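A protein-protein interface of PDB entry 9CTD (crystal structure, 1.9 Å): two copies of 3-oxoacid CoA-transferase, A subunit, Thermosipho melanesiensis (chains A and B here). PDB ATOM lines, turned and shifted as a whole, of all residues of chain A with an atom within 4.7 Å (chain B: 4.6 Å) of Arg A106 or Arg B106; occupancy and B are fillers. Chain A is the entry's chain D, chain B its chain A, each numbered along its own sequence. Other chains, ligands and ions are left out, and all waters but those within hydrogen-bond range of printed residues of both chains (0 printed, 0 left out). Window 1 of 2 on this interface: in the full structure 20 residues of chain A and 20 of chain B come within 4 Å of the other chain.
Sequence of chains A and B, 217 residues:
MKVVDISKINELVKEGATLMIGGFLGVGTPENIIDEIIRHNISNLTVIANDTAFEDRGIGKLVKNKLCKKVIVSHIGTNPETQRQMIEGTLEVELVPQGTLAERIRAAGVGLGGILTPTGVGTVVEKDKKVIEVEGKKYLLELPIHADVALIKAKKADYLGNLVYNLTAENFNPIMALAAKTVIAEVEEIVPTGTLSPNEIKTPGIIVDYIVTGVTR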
ATOM      1  N   ALA A 102      27.249 -15.963 -21.527  1.00  0.00           N
ATOM      2  CA  ALA A 102      26.120 -16.873 -21.581  1.00  0.00           C
ATOM      3  C   ALA A 102      25.784 -17.244 -23.012  1.00  0.00           C
ATOM      4  O   ALA A 102      25.535 -18.413 -23.311  1.00  0.00           O
ATOM      5  CB  ALA A 102      24.909 -16.244 -20.888  1.00  0.00           C
ATOM      6  N   GLU A 103      25.733 -16.262 -23.912  1.00  0.00           N
ATOM      7  CA  GLU A 103      25.337 -16.550 -25.282  1.00  0.00           C
ATOM      8  C   GLU A 103      26.438 -17.247 -26.070  1.00  0.00           C
ATOM      9  O   GLU A 103      26.135 -18.025 -26.978  1.00  0.00           O
ATOM     10  CB  GLU A 103      24.915 -15.267 -25.993  1.00  0.00           C
ATOM     11  CG  GLU A 103      23.583 -14.703 -25.492  1.00  0.00           C
ATOM     12  CD  GLU A 103      22.427 -15.648 -25.710  1.00  0.00           C
ATOM     13  OE1 GLU A 103      22.311 -16.118 -26.849  1.00  0.00           O
ATOM     14  OE2 GLU A 103      21.632 -15.891 -24.745  1.00  0.00           O
ATOM     15  N   ARG A 104      27.710 -16.961 -25.779  1.00  0.00           N
ATOM     16  CA  ARG A 104      28.801 -17.637 -26.483  1.00  0.00           C
ATOM     17  C   ARG A 104      28.875 -19.123 -26.091  1.00  0.00           C
ATOM     18  O   ARG A 104      29.087 -19.990 -26.945  1.00  0.00           O
ATOM     19  CB  ARG A 104      30.136 -16.935 -26.167  1.00  0.00           C
ATOM     20  CG  ARG A 104      30.327 -15.554 -26.812  1.00  0.00           C
ATOM     21  CD  ARG A 104      31.691 -14.959 -26.406  1.00  0.00           C
ATOM     22  NE  ARG A 104      32.800 -15.663 -27.029  1.00  0.00           N
ATOM     23  CZ  ARG A 104      34.075 -15.539 -26.680  1.00  0.00           C
ATOM     24  NH1 ARG A 104      34.457 -14.661 -25.777  1.00  0.00           N
ATOM     25  NH2 ARG A 104      34.989 -16.331 -27.255  1.00  0.00           N
ATOM     26  N   ILE A 105      28.716 -19.425 -24.799  1.00  0.00           N
ATOM     27  CA  ILE A 105      28.630 -20.819 -24.357  1.00  0.00           C
ATOM     28  C   ILE A 105      27.404 -21.484 -24.973  1.00  0.00           C
ATOM     29  O   ILE A 105      27.480 -22.581 -25.544  1.00  0.00           O
ATOM     30  CB  ILE A 105      28.593 -20.886 -22.820  1.00  0.00           C
ATOM     31  CG1 ILE A 105      29.882 -20.338 -22.234  1.00  0.00           C
ATOM     32  CG2 ILE A 105      28.375 -22.322 -22.345  1.00  0.00           C
ATOM     33  CD1 ILE A 105      29.859 -20.203 -20.698  1.00  0.00           C
ATOM     34  N   ARG A 106      26.259 -20.798 -24.914  1.00  0.00           N
ATOM     35  CA  ARG A 106      25.047 -21.352 -25.502  1.00  0.00           C
ATOM     36  C   ARG A 106      25.228 -21.657 -26.980  1.00  0.00           C
ATOM     37  O   ARG A 106      24.756 -22.695 -27.479  1.00  0.00           O
ATOM     38  CB  ARG A 106      23.892 -20.378 -25.299  1.00  0.00           C
ATOM     39  CG  ARG A 106      22.596 -20.957 -25.803  1.00  0.00           C
ATOM     40  CD  ARG A 106      21.447 -19.933 -25.712  1.00  0.00           C
ATOM     41  NE  ARG A 106      20.229 -20.503 -26.262  1.00  0.00           N
ATOM     42  CZ  ARG A 106      19.889 -20.456 -27.545  1.00  0.00           C
ATOM     43  NH1 ARG A 106      20.629 -19.824 -28.439  1.00  0.00           N
ATOM     44  NH2 ARG A 106      18.786 -21.093 -27.946  1.00  0.00           N
ATOM     45  N   ALA A 107      25.879 -20.744 -27.711  1.00  0.00           N
ATOM     46  CA  ALA A 107      26.037 -20.941 -29.140  1.00  0.00           C
ATOM     47  C   ALA A 107      26.761 -22.249 -29.417  1.00  0.00           C
ATOM     48  O   ALA A 107      26.394 -22.978 -30.345  1.00  0.00           O
ATOM     49  CB  ALA A 107      26.794 -19.777 -29.774  1.00  0.00           C
ATOM     50  N   ALA A 108      27.820 -22.534 -28.647  1.00  0.00           N
ATOM     51  CA  ALA A 108      28.491 -23.820 -28.800  1.00  0.00           C
ATOM     52  C   ALA A 108      27.546 -24.967 -28.461  1.00  0.00           C
ATOM     53  O   ALA A 108      27.591 -26.024 -29.095  1.00  0.00           O
ATOM     54  CB  ALA A 108      29.742 -23.878 -27.935  1.00  0.00           C
ATOM     55  N   GLY A 109      26.689 -24.782 -27.462  1.00  0.00           N
ATOM     56  CA  GLY A 109      25.804 -25.863 -27.059  1.00  0.00           C
ATOM     57  C   GLY A 109      24.671 -26.142 -28.033  1.00  0.00           C
ATOM     58  O   GLY A 109      24.171 -27.275 -28.110  1.00  0.00           O
ATOM     59  N   VAL A 110      24.218 -25.123 -28.765  1.00  0.00           N
ATOM     60  CA  VAL A 110      23.066 -25.271 -29.638  1.00  0.00           C
ATOM     61  C   VAL A 110      23.455 -25.249 -31.109  1.00  0.00           C
ATOM     62  O   VAL A 110      22.575 -25.219 -31.971  1.00  0.00           O
ATOM     63  CB  VAL A 110      21.957 -24.240 -29.341  1.00  0.00           C
ATOM     64  CG1 VAL A 110      21.593 -24.263 -27.867  1.00  0.00           C
ATOM     65  CG2 VAL A 110      22.334 -22.799 -29.732  1.00  0.00           C
ATOM     66  N   LEU A 112      25.272 -22.976 -33.043  1.00  0.00           N
ATOM     67  CA  LEU A 112      25.410 -21.729 -33.777  1.00  0.00           C
ATOM     68  C   LEU A 112      26.884 -21.434 -34.028  1.00  0.00           C
ATOM     69  O   LEU A 112      27.763 -21.880 -33.284  1.00  0.00           O
ATOM     70  CB  LEU A 112      24.780 -20.563 -32.992  1.00  0.00           C
ATOM     71  CG  LEU A 112      23.271 -20.706 -32.752  1.00  0.00           C
ATOM     72  CD1 LEU A 112      22.752 -19.574 -31.838  1.00  0.00           C
ATOM     73  CD2 LEU A 112      22.538 -20.761 -34.081  1.00  0.00           C
ATOM     74  N   ILE A 175      23.445 -24.281 -19.343  1.00  0.00           N
ATOM     75  CA  ILE A 175      24.040 -23.827 -20.590  1.00  0.00           C
ATOM     76  C   ILE A 175      25.304 -24.623 -20.887  1.00  0.00           C
ATOM     77  O   ILE A 175      25.510 -25.096 -22.007  1.00  0.00           O
ATOM     78  CB  ILE A 175      24.349 -22.314 -20.543  1.00  0.00           C
ATOM     79  CG1 ILE A 175      23.229 -21.495 -19.903  1.00  0.00           C
ATOM     80  CG2 ILE A 175      24.566 -21.861 -21.938  1.00  0.00           C
ATOM     81  CD1 ILE A 175      23.704 -19.996 -19.696  1.00  0.00           C
ATOM     82  N   ALA B 102      13.081 -20.506 -34.730  1.00  0.00           N
ATOM     83  CA  ALA B 102      13.194 -20.405 -33.282  1.00  0.00           C
ATOM     84  C   ALA B 102      14.283 -19.422 -32.877  1.00  0.00           C
ATOM     85  O   ALA B 102      14.092 -18.601 -31.963  1.00  0.00           O
ATOM     86  CB  ALA B 102      13.480 -21.799 -32.683  1.00  0.00           C
ATOM     87  N   GLU B 103      15.456 -19.523 -33.489  1.00  0.00           N
ATOM     88  CA  GLU B 103      16.557 -18.678 -33.071  1.00  0.00           C
ATOM     89  C   GLU B 103      16.372 -17.242 -33.515  1.00  0.00           C
ATOM     90  O   GLU B 103      16.877 -16.330 -32.848  1.00  0.00           O
ATOM     91  CB  GLU B 103      17.880 -19.218 -33.595  1.00  0.00           C
ATOM     92  CG  GLU B 103      18.390 -20.509 -32.860  1.00  0.00           C
ATOM     93  CD  GLU B 103      18.601 -20.346 -31.387  1.00  0.00           C
ATOM     94  OE1 GLU B 103      19.363 -19.438 -31.028  1.00  0.00           O
ATOM     95  OE2 GLU B 103      18.085 -21.182 -30.605  1.00  0.00           O
ATOM     96  N   ARG B 104      15.693 -17.026 -34.647  1.00  0.00           N
ATOM     97  CA  ARG B 104      15.457 -15.655 -35.118  1.00  0.00           C
ATOM     98  C   ARG B 104      14.463 -14.930 -34.230  1.00  0.00           C
ATOM     99  O   ARG B 104      14.637 -13.739 -33.925  1.00  0.00           O
ATOM    100  CB  ARG B 104      14.949 -15.653 -36.555  1.00  0.00           C
ATOM    101  CG  ARG B 104      16.046 -16.014 -37.601  1.00  0.00           C
ATOM    102  CD  ARG B 104      15.516 -15.991 -39.027  1.00  0.00           C
ATOM    103  NE  ARG B 104      15.137 -14.645 -39.463  1.00  0.00           N
ATOM    104  CZ  ARG B 104      14.362 -14.393 -40.515  1.00  0.00           C
ATOM    105  NH1 ARG B 104      13.948 -15.354 -41.312  1.00  0.00           N
ATOM    106  NH2 ARG B 104      13.961 -13.146 -40.755  1.00  0.00           N
ATOM    107  N   ILE B 105      13.380 -15.615 -33.866  1.00  0.00           N
ATOM    108  CA  ILE B 105      12.441 -15.088 -32.879  1.00  0.00           C
ATOM    109  C   ILE B 105      13.143 -14.865 -31.548  1.00  0.00           C
ATOM    110  O   ILE B 105      13.068 -13.785 -30.958  1.00  0.00           O
ATOM    111  CB  ILE B 105      11.245 -16.045 -32.738  1.00  0.00           C
ATOM    112  CG1 ILE B 105      10.514 -16.130 -34.073  1.00  0.00           C
ATOM    113  CG2 ILE B 105      10.321 -15.584 -31.598  1.00  0.00           C
ATOM    114  CD1 ILE B 105       9.437 -17.187 -34.176  1.00  0.00           C
ATOM    115  N   ARG B 106      13.903 -15.872 -31.078  1.00  0.00           N
ATOM    116  CA  ARG B 106      14.602 -15.714 -29.808  1.00  0.00           C
ATOM    117  C   ARG B 106      15.575 -14.535 -29.844  1.00  0.00           C
ATOM    118  O   ARG B 106      15.701 -13.787 -28.860  1.00  0.00           O
ATOM    119  CB  ARG B 106      15.361 -17.002 -29.457  1.00  0.00           C
ATOM    120  CG  ARG B 106      16.197 -16.866 -28.215  1.00  0.00           C
ATOM    121  CD  ARG B 106      16.919 -18.164 -27.872  1.00  0.00           C
ATOM    122  NE  ARG B 106      17.633 -18.064 -26.609  1.00  0.00           N
ATOM    123  CZ  ARG B 106      18.785 -17.433 -26.441  1.00  0.00           C
ATOM    124  NH1 ARG B 106      19.436 -16.885 -27.468  1.00  0.00           N
ATOM    125  NH2 ARG B 106      19.291 -17.335 -25.215  1.00  0.00           N
ATOM    126  N   ALA B 107      16.280 -14.347 -30.967  1.00  0.00           N
ATOM    127  CA  ALA B 107      17.220 -13.232 -31.040  1.00  0.00           C
ATOM    128  C   ALA B 107      16.515 -11.904 -30.754  1.00  0.00           C
ATOM    129  O   ALA B 107      17.057 -11.039 -30.046  1.00  0.00           O
ATOM    130  CB  ALA B 107      17.889 -13.194 -32.423  1.00  0.00           C
ATOM    131  N   ALA B 108      15.325 -11.722 -31.315  1.00  0.00           N
ATOM    132  CA  ALA B 108      14.559 -10.511 -31.044  1.00  0.00           C
ATOM    133  C   ALA B 108      14.186 -10.416 -29.576  1.00  0.00           C
ATOM    134  O   ALA B 108      14.192  -9.322 -28.990  1.00  0.00           O
ATOM    135  CB  ALA B 108      13.306 -10.480 -31.910  1.00  0.00           C
ATOM    136  N   GLY B 109      13.821 -11.548 -28.974  1.00  0.00           N
ATOM    137  CA  GLY B 109      13.408 -11.555 -27.586  1.00  0.00           C
ATOM    138  C   GLY B 109      14.521 -11.287 -26.586  1.00  0.00           C
ATOM    139  O   GLY B 109      14.268 -10.744 -25.506  1.00  0.00           O
ATOM    140  N   VAL B 110      15.751 -11.688 -26.898  1.00  0.00           N
ATOM    141  CA  VAL B 110      16.855 -11.587 -25.958  1.00  0.00           C
ATOM    142  C   VAL B 110      17.838 -10.489 -26.349  1.00  0.00           C
ATOM    143  O   VAL B 110      18.872 -10.339 -25.702  1.00  0.00           O
ATOM    144  CB  VAL B 110      17.592 -12.929 -25.785  1.00  0.00           C
ATOM    145  CG1 VAL B 110      16.623 -13.994 -25.316  1.00  0.00           C
ATOM    146  CG2 VAL B 110      18.330 -13.356 -27.063  1.00  0.00           C
ATOM    147  N   LEU B 112      19.606  -9.812 -29.311  1.00  0.00           N
ATOM    148  CA  LEU B 112      20.714 -10.058 -30.220  1.00  0.00           C
ATOM    149  C   LEU B 112      20.410  -9.419 -31.567  1.00  0.00           C
ATOM    150  O   LEU B 112      19.252  -9.205 -31.927  1.00  0.00           O
ATOM    151  CB  LEU B 112      20.927 -11.555 -30.397  1.00  0.00           C
ATOM    152  CG  LEU B 112      21.342 -12.347 -29.163  1.00  0.00           C
ATOM    153  CD1 LEU B 112      21.388 -13.884 -29.470  1.00  0.00           C
ATOM    154  CD2 LEU B 112      22.653 -11.827 -28.651  1.00  0.00           C
ATOM    155  N   ILE B 175       9.208 -18.533 -26.368  1.00  0.00           N
ATOM    156  CA  ILE B 175      10.109 -17.755 -27.208  1.00  0.00           C
ATOM    157  C   ILE B 175       9.405 -16.515 -27.726  1.00  0.00           C
ATOM    158  O   ILE B 175       9.958 -15.417 -27.664  1.00  0.00           O
ATOM    159  CB  ILE B 175      10.652 -18.591 -28.393  1.00  0.00           C
ATOM    160  CG1 ILE B 175      10.834 -20.065 -27.983  1.00  0.00           C
ATOM    161  CG2 ILE B 175      11.889 -17.880 -28.970  1.00  0.00           C
ATOM    162  CD1 ILE B 175      11.382 -20.887 -29.201  1.00  0.00           C
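Glu A103 touches Arg B106, and with the chains exchanged Arg A106 touches Glu B103.
Glu A103 touches Leu B112, and with the chains exchanged Leu A112 touches Glu B103.
Arg B106 touches its own counterpart, Arg A106.
Of the 5 pairs that touch across the chains among the printed residues, 5 have their exchanged pair printed and touching as well.
Leu B112 touches Glu A103 (CD1 to OE1, 3.6 Å).
Glu B103 touches Leu A112 (OE1 to CD1, 3.5 Å).
The backbone carbonyl oxygen (O) of Ala A107 lies within hydrogen-bond range of the backbone NH (N) of Leu A112, 2.9 Å away.
O of Ala B107 sits at hydrogen-bond distance from N of Leu B112 (2.9 Å).
Printed residues of chain A that touch a printed residue of chain B: Glu A103, Arg A106 and Leu A112.
Hydrophobic or aromatic side chains of chain A that line the printed part of chain B: Leu A112.
Hydrophobic or aromatic side chains of chain B that line the printed part of chain A: Leu B112.
Among the printed residues, 5 pairs touch across the chains.
The side-chain carboxylate of Glu A103 is in salt-bridge range of the guanidinium group of Arg B106 (2.8 Å).
The side-chain carboxylate (OE2) of Glu B103 lies within salt-bridge range of the guanidinium group (NH2) of Arg A106 (2.8 Å).
The guanidinium group of Arg B106 lies close to the guanidinium group of Arg A106, at 3.3 Å.
Arg A106 touches just these residues of chain B: Glu B103 and Arg B106.
Printed residues of chain B within 4 Å of Glu A103: Arg B106 (2.8 Å) and Leu B112 (3.6 Å).
Printed residues of chain A within 4 Å of Glu B103: Arg A106 and Leu A112.
Ala A107 touches none of the printed residues of chain B.
The nearest printed residue of chain A that does not touch Glu B103 is Val A110 (4.6 Å).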
